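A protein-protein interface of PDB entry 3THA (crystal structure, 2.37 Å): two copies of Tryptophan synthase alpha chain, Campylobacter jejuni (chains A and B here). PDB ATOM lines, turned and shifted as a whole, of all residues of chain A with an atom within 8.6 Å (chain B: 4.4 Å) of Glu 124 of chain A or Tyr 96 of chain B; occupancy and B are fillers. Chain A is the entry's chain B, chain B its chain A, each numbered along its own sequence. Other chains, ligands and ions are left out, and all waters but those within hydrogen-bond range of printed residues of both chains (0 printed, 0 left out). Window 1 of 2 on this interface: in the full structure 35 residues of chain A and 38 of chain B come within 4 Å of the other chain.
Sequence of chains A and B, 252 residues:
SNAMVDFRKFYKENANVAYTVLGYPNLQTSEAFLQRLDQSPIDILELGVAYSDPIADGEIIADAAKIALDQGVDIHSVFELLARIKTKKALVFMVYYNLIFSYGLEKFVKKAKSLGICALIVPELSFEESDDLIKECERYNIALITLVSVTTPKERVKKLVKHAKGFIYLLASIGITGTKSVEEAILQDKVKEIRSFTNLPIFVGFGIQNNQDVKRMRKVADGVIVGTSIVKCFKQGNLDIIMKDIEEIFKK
The side-chain hydroxyl (OG) of Ser 52 of chain B lies within hydrogen-bond range of the side-chain carboxylate (OE1) of Glu 124 of chain A (2.6 Å).
The side-chain amide nitrogen (ND2) of Asn 98 of chain A sits at hydrogen-bond distance from the side-chain carboxylate (OE1) of Glu 124 of chain B, 3.1 Å away.
The side-chain amide nitrogen (ND2) of Asn 98 of chain B sits at hydrogen-bond distance from the backbone carbonyl oxygen (O) of Glu 124 of chain A (3.0 Å).
OG of Ser 126 of chain A is in hydrogen-bond range of OE2 of Glu 129 of chain A (3.2 Å).
Among the printed residues, merely in contact across the chains: Ile 55 of chain A with Pro 123 of chain B, Met 94 of chain A with Ile 55 of chain B, Tyr 96 of chain A with Glu 124 of chain B, Pro 123 of chain A with Ile 55 of chain B, Glu 124 of chain A with Ile 55 of chain B, Glu 124 of chain A with Tyr 96 of chain B, Glu 129 of chain A with Tyr 97 of chain B, Glu 129 of chain A with Asn 98 of chain B, Leu 147 of chain A with Ile 55 of chain B and Leu 171 of chain A with Ile 55 of chain B.
Of the printed residues of chain B, Tyr 96 of chain A touches Glu 124 (3.7 Å).
Of chain B, only Ser 52 (2.6 Å), Ile 55 (3.9 Å), Tyr 96 (3.8 Å) and Asn 98 (3.0 Å) come within 4 Å of Glu 124 of chain A.
Of the printed residues of chain A, Ser 52 of chain B touches Glu 124.
Of chain A, only Glu 124 comes within 4 Å of Tyr 96 of chain B.
The nearest printed residue of chain B that does not touch Glu 124 of chain A is Tyr 97 of chain B (5.9 Å).
The nearest residue of chain A that does not touch Tyr 96 of chain B is Tyr 96 of chain A (4.4 Å).
The nearest printed residue of chain A that does not touch Glu 124 of chain B is Pro 54 of chain A (4.1 Å).
Printed residues of chain A that touch a printed residue of chain B: Ile 55, Met 94, Tyr 96, Asn 98, Pro 123, Glu 124, Glu 129, Leu 147 and Leu 171.
Hydrophobic or aromatic side chains of chain A within 4 Å of the printed part of chain B: Ile 55, Met 94, Tyr 96, Pro 123, Leu 147 and Leu 171.
Hydrophobic or aromatic side chains of chain B within 4 Å of the printed part of chain A: Ile 55, Tyr 96, Tyr 97 and Pro 123.
Among the printed residues, 13 pairs touch across the chains.
Ile 55 of chain A touches Pro 123 of chain B, and with the chains exchanged Pro 123 of chain A touches Ile 55 of chain B.
Tyr 96 of chain A touches Glu 124 of chain B, and with the chains exchanged Glu 124 of chain A touches Tyr 96 of chain B.
Asn 98 of chain A touches Glu 124 of chain B, and with the chains exchanged Glu 124 of chain A touches Asn 98 of chain B.
Glu 124 of chain A touches Ile 55 of chain B, but with the chains exchanged Ile 55 of chain A does not touch Glu 124 of chain B (4.2 Å).
Positions printed for both chains: 55, 95, 96, 97, 98, 122, 123 and 124.
Of the 13 pairs that touch across the chains among the printed residues, 6 have their exchanged pair printed and touching as well.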
ATOM      1  N   PRO A  54     -23.092  27.821   1.992  1.00  0.00           N
ATOM      2  CA  PRO A  54     -23.773  26.557   2.325  1.00  0.00           C
ATOM      3  C   PRO A  54     -25.283  26.536   2.195  1.00  0.00           C
ATOM      4  O   PRO A  54     -25.987  27.337   2.791  1.00  0.00           O
ATOM      5  CB  PRO A  54     -23.388  26.347   3.770  1.00  0.00           C
ATOM      6  CG  PRO A  54     -21.947  26.860   3.779  1.00  0.00           C
ATOM      7  CD  PRO A  54     -21.918  28.041   2.862  1.00  0.00           C
ATOM      8  N   ILE A  55     -25.754  25.558   1.437  1.00  0.00           N
ATOM      9  CA  ILE A  55     -27.139  25.406   1.066  1.00  0.00           C
ATOM     10  C   ILE A  55     -28.015  24.893   2.192  1.00  0.00           C
ATOM     11  O   ILE A  55     -29.248  24.984   2.131  1.00  0.00           O
ATOM     12  CB  ILE A  55     -27.224  24.421  -0.088  1.00  0.00           C
ATOM     13  CG1 ILE A  55     -28.555  24.564  -0.806  1.00  0.00           C
ATOM     14  CG2 ILE A  55     -26.977  23.002   0.417  1.00  0.00           C
ATOM     15  CD1 ILE A  55     -28.448  24.233  -2.273  1.00  0.00           C
ATOM     16  N   ALA A  56     -27.370  24.291   3.176  1.00  0.00           N
ATOM     17  CA  ALA A  56     -27.973  23.858   4.443  1.00  0.00           C
ATOM     18  C   ALA A  56     -29.246  24.615   4.963  1.00  0.00           C
ATOM     19  O   ALA A  56     -29.724  25.574   4.330  1.00  0.00           O
ATOM     20  CB  ALA A  56     -26.863  23.884   5.488  1.00  0.00           C
ATOM     21  N   GLU A  59     -27.766  25.169  10.290  1.00  0.00           N
ATOM     22  CA  GLU A  59     -26.635  24.496  10.964  1.00  0.00           C
ATOM     23  C   GLU A  59     -25.462  25.317  11.519  1.00  0.00           C
ATOM     24  O   GLU A  59     -24.994  26.275  10.897  1.00  0.00           O
ATOM     25  CB  GLU A  59     -26.053  23.341  10.106  1.00  0.00           C
ATOM     26  CG  GLU A  59     -26.405  23.318   8.635  1.00  0.00           C
ATOM     27  CD  GLU A  59     -27.620  22.450   8.292  1.00  0.00           C
ATOM     28  OE1 GLU A  59     -27.513  21.200   8.167  1.00  0.00           O
ATOM     29  OE2 GLU A  59     -28.684  23.019   8.079  1.00  0.00           O
ATOM     30  N   MET A  94      -9.926  21.415   4.946  1.00  0.00           N
ATOM     31  CA  MET A  94     -11.131  20.706   4.620  1.00  0.00           C
ATOM     32  C   MET A  94     -11.962  21.744   3.885  1.00  0.00           C
ATOM     33  O   MET A  94     -12.430  22.680   4.477  1.00  0.00           O
ATOM     34  CB  MET A  94     -11.794  20.180   5.879  1.00  0.00           C
ATOM     35  CG  MET A  94     -13.152  19.609   5.716  1.00  0.00           C
ATOM     36  SD  MET A  94     -13.333  18.334   7.184  1.00  0.00           S
ATOM     37  CE  MET A  94     -15.174  17.937   7.068  1.00  0.00           C
ATOM     38  N   VAL A  95     -12.071  21.594   2.574  1.00  0.00           N
ATOM     39  CA  VAL A  95     -12.838  22.483   1.720  1.00  0.00           C
ATOM     40  C   VAL A  95     -13.626  21.647   0.720  1.00  0.00           C
ATOM     41  O   VAL A  95     -13.264  20.533   0.419  1.00  0.00           O
ATOM     42  CB  VAL A  95     -11.889  23.431   0.885  1.00  0.00           C
ATOM     43  CG1 VAL A  95     -11.196  24.434   1.775  1.00  0.00           C
ATOM     44  CG2 VAL A  95     -10.866  22.640   0.121  1.00  0.00           C
ATOM     45  N   TYR A  96     -14.692  22.208   0.191  1.00  0.00           N
ATOM     46  CA  TYR A  96     -15.348  21.604  -0.937  1.00  0.00           C
ATOM     47  C   TYR A  96     -14.554  21.878  -2.173  1.00  0.00           C
ATOM     48  O   TYR A  96     -13.777  22.843  -2.215  1.00  0.00           O
ATOM     49  CB  TYR A  96     -16.686  22.205  -1.106  1.00  0.00           C
ATOM     50  CG  TYR A  96     -17.651  21.763  -0.068  1.00  0.00           C
ATOM     51  CD1 TYR A  96     -18.245  20.536  -0.170  1.00  0.00           C
ATOM     52  CD2 TYR A  96     -17.975  22.574   1.022  1.00  0.00           C
ATOM     53  CE1 TYR A  96     -19.155  20.122   0.725  1.00  0.00           C
ATOM     54  CE2 TYR A  96     -18.902  22.148   1.955  1.00  0.00           C
ATOM     55  CZ  TYR A  96     -19.496  20.908   1.778  1.00  0.00           C
ATOM     56  OH  TYR A  96     -20.442  20.394   2.641  1.00  0.00           O
ATOM     57  N   TYR A  97     -14.719  20.997  -3.146  1.00  0.00           N
ATOM     58  CA  TYR A  97     -13.990  21.031  -4.397  1.00  0.00           C
ATOM     59  C   TYR A  97     -14.218  22.312  -5.194  1.00  0.00           C
ATOM     60  O   TYR A  97     -13.329  22.738  -5.941  1.00  0.00           O
ATOM     61  CB  TYR A  97     -14.340  19.810  -5.246  1.00  0.00           C
ATOM     62  CG  TYR A  97     -13.376  19.561  -6.393  1.00  0.00           C
ATOM     63  CD1 TYR A  97     -12.167  18.907  -6.186  1.00  0.00           C
ATOM     64  CD2 TYR A  97     -13.691  19.953  -7.690  1.00  0.00           C
ATOM     65  CE1 TYR A  97     -11.285  18.664  -7.235  1.00  0.00           C
ATOM     66  CE2 TYR A  97     -12.833  19.701  -8.742  1.00  0.00           C
ATOM     67  CZ  TYR A  97     -11.621  19.068  -8.506  1.00  0.00           C
ATOM     68  OH  TYR A  97     -10.758  18.820  -9.556  1.00  0.00           O
ATOM     69  N   ASN A  98     -15.389  22.928  -5.031  1.00  0.00           N
ATOM     70  CA  ASN A  98     -15.715  24.133  -5.759  1.00  0.00           C
ATOM     71  C   ASN A  98     -14.713  25.252  -5.473  1.00  0.00           C
ATOM     72  O   ASN A  98     -14.422  26.060  -6.344  1.00  0.00           O
ATOM     73  CB  ASN A  98     -17.146  24.592  -5.494  1.00  0.00           C
ATOM     74  CG  ASN A  98     -17.439  24.885  -3.996  1.00  0.00           C
ATOM     75  OD1 ASN A  98     -16.563  25.251  -3.201  1.00  0.00           O
ATOM     76  ND2 ASN A  98     -18.685  24.724  -3.626  1.00  0.00           N
ATOM     77  N   ILE A 121      -8.855  17.374   2.946  1.00  0.00           N
ATOM     78  CA  ILE A 121     -10.024  16.550   2.986  1.00  0.00           C
ATOM     79  C   ILE A 121     -11.074  17.268   2.119  1.00  0.00           C
ATOM     80  O   ILE A 121     -11.407  18.428   2.383  1.00  0.00           O
ATOM     81  CB  ILE A 121     -10.576  16.496   4.404  1.00  0.00           C
ATOM     82  CG1 ILE A 121      -9.482  16.108   5.400  1.00  0.00           C
ATOM     83  CG2 ILE A 121     -11.812  15.572   4.501  1.00  0.00           C
ATOM     84  CD1 ILE A 121      -9.926  16.184   6.843  1.00  0.00           C
ATOM     85  N   VAL A 122     -11.619  16.598   1.104  1.00  0.00           N
ATOM     86  CA  VAL A 122     -12.607  17.235   0.232  1.00  0.00           C
ATOM     87  C   VAL A 122     -13.912  16.460   0.344  1.00  0.00           C
ATOM     88  O   VAL A 122     -14.043  15.353  -0.227  1.00  0.00           O
ATOM     89  CB  VAL A 122     -12.144  17.314  -1.249  1.00  0.00           C
ATOM     90  CG1 VAL A 122     -13.088  18.205  -2.027  1.00  0.00           C
ATOM     91  CG2 VAL A 122     -10.652  17.865  -1.369  1.00  0.00           C
ATOM     92  N   PRO A 123     -14.856  17.001   1.136  1.00  0.00           N
ATOM     93  CA  PRO A 123     -16.118  16.357   1.324  1.00  0.00           C
ATOM     94  C   PRO A 123     -16.805  16.271  -0.009  1.00  0.00           C
ATOM     95  O   PRO A 123     -16.776  17.250  -0.799  1.00  0.00           O
ATOM     96  CB  PRO A 123     -16.913  17.374   2.214  1.00  0.00           C
ATOM     97  CG  PRO A 123     -15.850  18.106   2.921  1.00  0.00           C
ATOM     98  CD  PRO A 123     -14.750  18.250   1.927  1.00  0.00           C
ATOM     99  N   GLU A 124     -17.482  15.140  -0.193  1.00  0.00           N
ATOM    100  CA  GLU A 124     -18.321  14.849  -1.332  1.00  0.00           C
ATOM    101  C   GLU A 124     -17.545  14.756  -2.659  1.00  0.00           C
ATOM    102  O   GLU A 124     -18.164  14.610  -3.738  1.00  0.00           O
ATOM    103  CB  GLU A 124     -19.514  15.793  -1.418  1.00  0.00           C
ATOM    104  CG  GLU A 124     -20.214  16.066  -0.061  1.00  0.00           C
ATOM    105  CD  GLU A 124     -20.935  14.852   0.549  1.00  0.00           C
ATOM    106  OE1 GLU A 124     -20.975  13.754  -0.091  1.00  0.00           O
ATOM    107  OE2 GLU A 124     -21.444  15.023   1.688  1.00  0.00           O
ATOM    108  N   LEU A 125     -16.209  14.772  -2.584  1.00  0.00           N
ATOM    109  CA  LEU A 125     -15.426  14.382  -3.750  1.00  0.00           C
ATOM    110  C   LEU A 125     -15.208  12.887  -3.646  1.00  0.00           C
ATOM    111  O   LEU A 125     -14.391  12.442  -2.846  1.00  0.00           O
ATOM    112  CB  LEU A 125     -14.102  15.122  -3.834  1.00  0.00           C
ATOM    113  CG  LEU A 125     -13.289  14.961  -5.122  1.00  0.00           C
ATOM    114  CD1 LEU A 125     -13.979  15.663  -6.280  1.00  0.00           C
ATOM    115  CD2 LEU A 125     -11.920  15.559  -4.910  1.00  0.00           C
ATOM    116  N   SER A 126     -15.946  12.099  -4.416  1.00  0.00           N
ATOM    117  CA  SER A 126     -15.727  10.649  -4.387  1.00  0.00           C
ATOM    118  C   SER A 126     -14.363  10.277  -4.991  1.00  0.00           C
ATOM    119  O   SER A 126     -13.724  11.071  -5.710  1.00  0.00           O
ATOM    120  CB  SER A 126     -16.812   9.892  -5.165  1.00  0.00           C
ATOM    121  OG  SER A 126     -16.598  10.086  -6.549  1.00  0.00           O
ATOM    122  N   PHE A 127     -13.931   9.049  -4.715  1.00  0.00           N
ATOM    123  CA  PHE A 127     -12.626   8.613  -5.190  1.00  0.00           C
ATOM    124  C   PHE A 127     -12.510   8.698  -6.724  1.00  0.00           C
ATOM    125  O   PHE A 127     -11.490   9.130  -7.289  1.00  0.00           O
ATOM    126  CB  PHE A 127     -12.363   7.191  -4.729  1.00  0.00           C
ATOM    127  CG  PHE A 127     -11.084   6.626  -5.273  1.00  0.00           C
ATOM    128  CD1 PHE A 127     -11.097   5.847  -6.443  1.00  0.00           C
ATOM    129  CD2 PHE A 127      -9.857   6.934  -4.659  1.00  0.00           C
ATOM    130  CE1 PHE A 127      -9.905   5.351  -6.967  1.00  0.00           C
ATOM    131  CE2 PHE A 127      -8.649   6.446  -5.175  1.00  0.00           C
ATOM    132  CZ  PHE A 127      -8.669   5.651  -6.334  1.00  0.00           C
ATOM    133  N   GLU A 129     -13.850  10.687  -8.738  1.00  0.00           N
ATOM    134  CA  GLU A 129     -13.799  12.060  -9.253  1.00  0.00           C
ATOM    135  C   GLU A 129     -12.463  12.684  -8.960  1.00  0.00           C
ATOM    136  O   GLU A 129     -12.132  13.735  -9.489  1.00  0.00           O
ATOM    137  CB  GLU A 129     -14.872  12.942  -8.611  1.00  0.00           C
ATOM    138  CG  GLU A 129     -16.254  12.807  -9.168  1.00  0.00           C
ATOM    139  CD  GLU A 129     -17.265  13.565  -8.321  1.00  0.00           C
ATOM    140  OE1 GLU A 129     -17.429  14.805  -8.503  1.00  0.00           O
ATOM    141  OE2 GLU A 129     -17.888  12.916  -7.451  1.00  0.00           O
ATOM    142  N   SER A 130     -11.694  12.023  -8.112  1.00  0.00           N
ATOM    143  CA  SER A 130     -10.476  12.598  -7.564  1.00  0.00           C
ATOM    144  C   SER A 130      -9.253  12.673  -8.459  1.00  0.00           C
ATOM    145  O   SER A 130      -8.274  13.308  -8.080  1.00  0.00           O
ATOM    146  CB  SER A 130     -10.112  11.844  -6.292  1.00  0.00           C
ATOM    147  OG  SER A 130     -11.163  11.967  -5.337  1.00  0.00           O
ATOM    148  N   LEU A 147     -11.704   8.631   2.972  1.00  0.00           N
ATOM    149  CA  LEU A 147     -12.800   8.469   3.887  1.00  0.00           C
ATOM    150  C   LEU A 147     -13.361   7.102   3.796  1.00  0.00           C
ATOM    151  O   LEU A 147     -13.546   6.607   2.700  1.00  0.00           O
ATOM    152  CB  LEU A 147     -13.919   9.443   3.529  1.00  0.00           C
ATOM    153  CG  LEU A 147     -13.825  10.802   4.188  1.00  0.00           C
ATOM    154  CD1 LEU A 147     -12.433  11.474   3.984  1.00  0.00           C
ATOM    155  CD2 LEU A 147     -14.925  11.646   3.626  1.00  0.00           C
ATOM    156  N   LEU A 171     -15.435   7.507   9.335  1.00  0.00           N
ATOM    157  CA  LEU A 171     -16.674   8.076   9.827  1.00  0.00           C
ATOM    158  C   LEU A 171     -17.282   7.094  10.801  1.00  0.00           C
ATOM    159  O   LEU A 171     -17.024   5.889  10.737  1.00  0.00           O
ATOM    160  CB  LEU A 171     -17.643   8.396   8.690  1.00  0.00           C
ATOM    161  CG  LEU A 171     -17.034   9.331   7.648  1.00  0.00           C
ATOM    162  CD1 LEU A 171     -17.951   9.533   6.484  1.00  0.00           C
ATOM    163  CD2 LEU A 171     -16.693  10.650   8.260  1.00  0.00           C
ATOM    164  N   SER B  52     -23.257   9.177  -0.305  1.00  0.00           N
ATOM    165  CA  SER B  52     -22.154   8.990   0.670  1.00  0.00           C
ATOM    166  C   SER B  52     -22.566   9.412   2.094  1.00  0.00           C
ATOM    167  O   SER B  52     -23.519  10.213   2.268  1.00  0.00           O
ATOM    168  CB  SER B  52     -20.926   9.822   0.240  1.00  0.00           C
ATOM    169  OG  SER B  52     -21.187  11.221   0.333  1.00  0.00           O
ATOM    170  N   ILE B  55     -19.677  14.242   6.864  1.00  0.00           N
ATOM    171  CA  ILE B  55     -18.300  14.229   7.309  1.00  0.00           C
ATOM    172  C   ILE B  55     -18.004  14.732   8.728  1.00  0.00           C
ATOM    173  O   ILE B  55     -17.937  13.908   9.633  1.00  0.00           O
ATOM    174  CB  ILE B  55     -17.373  14.905   6.290  1.00  0.00           C
ATOM    175  CG1 ILE B  55     -18.122  15.274   4.991  1.00  0.00           C
ATOM    176  CG2 ILE B  55     -16.115  14.071   6.098  1.00  0.00           C
ATOM    177  CD1 ILE B  55     -18.451  14.123   3.973  1.00  0.00           C
ATOM    178  N   VAL B  95     -29.444  16.379  -4.769  1.00  0.00           N
ATOM    179  CA  VAL B  95     -28.436  15.335  -4.681  1.00  0.00           C
ATOM    180  C   VAL B  95     -27.053  15.934  -4.917  1.00  0.00           C
ATOM    181  O   VAL B  95     -26.916  16.891  -5.719  1.00  0.00           O
ATOM    182  CB  VAL B  95     -28.694  14.218  -5.739  1.00  0.00           C
ATOM    183  CG1 VAL B  95     -30.117  13.614  -5.580  1.00  0.00           C
ATOM    184  CG2 VAL B  95     -28.534  14.810  -7.162  1.00  0.00           C
ATOM    185  N   TYR B  96     -26.021  15.359  -4.286  1.00  0.00           N
ATOM    186  CA  TYR B  96     -24.629  15.748  -4.633  1.00  0.00           C
ATOM    187  C   TYR B  96     -24.236  15.241  -6.001  1.00  0.00           C
ATOM    188  O   TYR B  96     -24.843  14.274  -6.520  1.00  0.00           O
ATOM    189  CB  TYR B  96     -23.604  15.313  -3.582  1.00  0.00           C
ATOM    190  CG  TYR B  96     -23.746  16.104  -2.291  1.00  0.00           C
ATOM    191  CD1 TYR B  96     -23.213  17.394  -2.182  1.00  0.00           C
ATOM    192  CD2 TYR B  96     -24.414  15.581  -1.203  1.00  0.00           C
ATOM    193  CE1 TYR B  96     -23.322  18.138  -1.009  1.00  0.00           C
ATOM    194  CE2 TYR B  96     -24.529  16.325  -0.009  1.00  0.00           C
ATOM    195  CZ  TYR B  96     -23.984  17.612   0.059  1.00  0.00           C
ATOM    196  OH  TYR B  96     -24.070  18.367   1.216  1.00  0.00           O
ATOM    197  N   TYR B  97     -23.233  15.902  -6.587  1.00  0.00           N
ATOM    198  CA  TYR B  97     -22.825  15.628  -7.919  1.00  0.00           C
ATOM    199  C   TYR B  97     -22.268  14.241  -8.010  1.00  0.00           C
ATOM    200  O   TYR B  97     -22.413  13.615  -9.071  1.00  0.00           O
ATOM    201  CB  TYR B  97     -21.783  16.613  -8.387  1.00  0.00           C
ATOM    202  CG  TYR B  97     -21.465  16.519  -9.886  1.00  0.00           C
ATOM    203  CD1 TYR B  97     -22.410  16.854 -10.848  1.00  0.00           C
ATOM    204  CD2 TYR B  97     -20.201  16.128 -10.321  1.00  0.00           C
ATOM    205  CE1 TYR B  97     -22.106  16.807 -12.187  1.00  0.00           C
ATOM    206  CE2 TYR B  97     -19.870  16.077 -11.681  1.00  0.00           C
ATOM    207  CZ  TYR B  97     -20.823  16.426 -12.608  1.00  0.00           C
ATOM    208  OH  TYR B  97     -20.496  16.385 -13.938  1.00  0.00           O
ATOM    209  N   ASN B  98     -21.664  13.751  -6.916  1.00  0.00           N
ATOM    210  CA  ASN B  98     -21.045  12.426  -6.927  1.00  0.00           C
ATOM    211  C   ASN B  98     -22.035  11.307  -7.288  1.00  0.00           C
ATOM    212  O   ASN B  98     -21.674  10.309  -7.853  1.00  0.00           O
ATOM    213  CB  ASN B  98     -20.257  12.090  -5.620  1.00  0.00           C
ATOM    214  CG  ASN B  98     -21.081  12.284  -4.304  1.00  0.00           C
ATOM    215  OD1 ASN B  98     -22.282  12.041  -4.246  1.00  0.00           O
ATOM    216  ND2 ASN B  98     -20.384  12.688  -3.222  1.00  0.00           N
ATOM    217  N   LEU B  99     -23.282  11.497  -6.936  1.00  0.00           N
ATOM    218  CA  LEU B  99     -24.282  10.478  -7.109  1.00  0.00           C
ATOM    219  C   LEU B  99     -24.710  10.538  -8.578  1.00  0.00           C
ATOM    220  O   LEU B  99     -25.082   9.545  -9.133  1.00  0.00           O
ATOM    221  CB  LEU B  99     -25.449  10.751  -6.158  1.00  0.00           C
ATOM    222  CG  LEU B  99     -26.639   9.814  -6.129  1.00  0.00           C
ATOM    223  CD1 LEU B  99     -27.439   9.906  -4.804  1.00  0.00           C
ATOM    224  CD2 LEU B  99     -27.593  10.025  -7.281  1.00  0.00           C
ATOM    225  N   ILE B 100     -24.623  11.705  -9.205  1.00  0.00           N
ATOM    226  CA  ILE B 100     -24.957  11.837 -10.640  1.00  0.00           C
ATOM    227  C   ILE B 100     -23.832  11.250 -11.531  1.00  0.00           C
ATOM    228  O   ILE B 100     -24.079  10.434 -12.466  1.00  0.00           O
ATOM    229  CB  ILE B 100     -25.226  13.310 -11.002  1.00  0.00           C
ATOM    230  CG1 ILE B 100     -26.525  13.781 -10.316  1.00  0.00           C
ATOM    231  CG2 ILE B 100     -25.277  13.461 -12.481  1.00  0.00           C
ATOM    232  CD1 ILE B 100     -26.843  15.257 -10.457  1.00  0.00           C
ATOM    233  N   VAL B 122     -28.194  20.842  -6.978  1.00  0.00           N
ATOM    234  CA  VAL B 122     -26.977  20.086  -6.764  1.00  0.00           C
ATOM    235  C   VAL B 122     -26.066  20.896  -5.892  1.00  0.00           C
ATOM    236  O   VAL B 122     -25.210  21.618  -6.375  1.00  0.00           O
ATOM    237  CB  VAL B 122     -26.323  19.644  -8.112  1.00  0.00           C
ATOM    238  CG1 VAL B 122     -25.106  18.735  -7.897  1.00  0.00           C
ATOM    239  CG2 VAL B 122     -27.377  18.865  -8.946  1.00  0.00           C
ATOM    240  N   PRO B 123     -26.213  20.728  -4.581  1.00  0.00           N
ATOM    241  CA  PRO B 123     -25.469  21.505  -3.607  1.00  0.00           C
ATOM    242  C   PRO B 123     -24.016  21.473  -3.982  1.00  0.00           C
ATOM    243  O   PRO B 123     -23.499  20.398  -4.329  1.00  0.00           O
ATOM    244  CB  PRO B 123     -25.606  20.686  -2.293  1.00  0.00           C
ATOM    245  CG  PRO B 123     -26.742  19.842  -2.483  1.00  0.00           C
ATOM    246  CD  PRO B 123     -26.796  19.525  -3.966  1.00  0.00           C
ATOM    247  N   GLU B 124     -23.358  22.616  -3.863  1.00  0.00           N
ATOM    248  CA  GLU B 124     -21.919  22.707  -3.966  1.00  0.00           C
ATOM    249  C   GLU B 124     -21.409  22.525  -5.390  1.00  0.00           C
ATOM    250  O   GLU B 124     -20.213  22.573  -5.592  1.00  0.00           O
ATOM    251  CB  GLU B 124     -21.177  21.715  -3.021  1.00  0.00           C
ATOM    252  CG  GLU B 124     -21.478  21.832  -1.529  1.00  0.00           C
ATOM    253  CD  GLU B 124     -21.583  23.291  -0.993  1.00  0.00           C
ATOM    254  OE1 GLU B 124     -20.746  24.187  -1.346  1.00  0.00           O
ATOM    255  OE2 GLU B 124     -22.512  23.507  -0.171  1.00  0.00           O
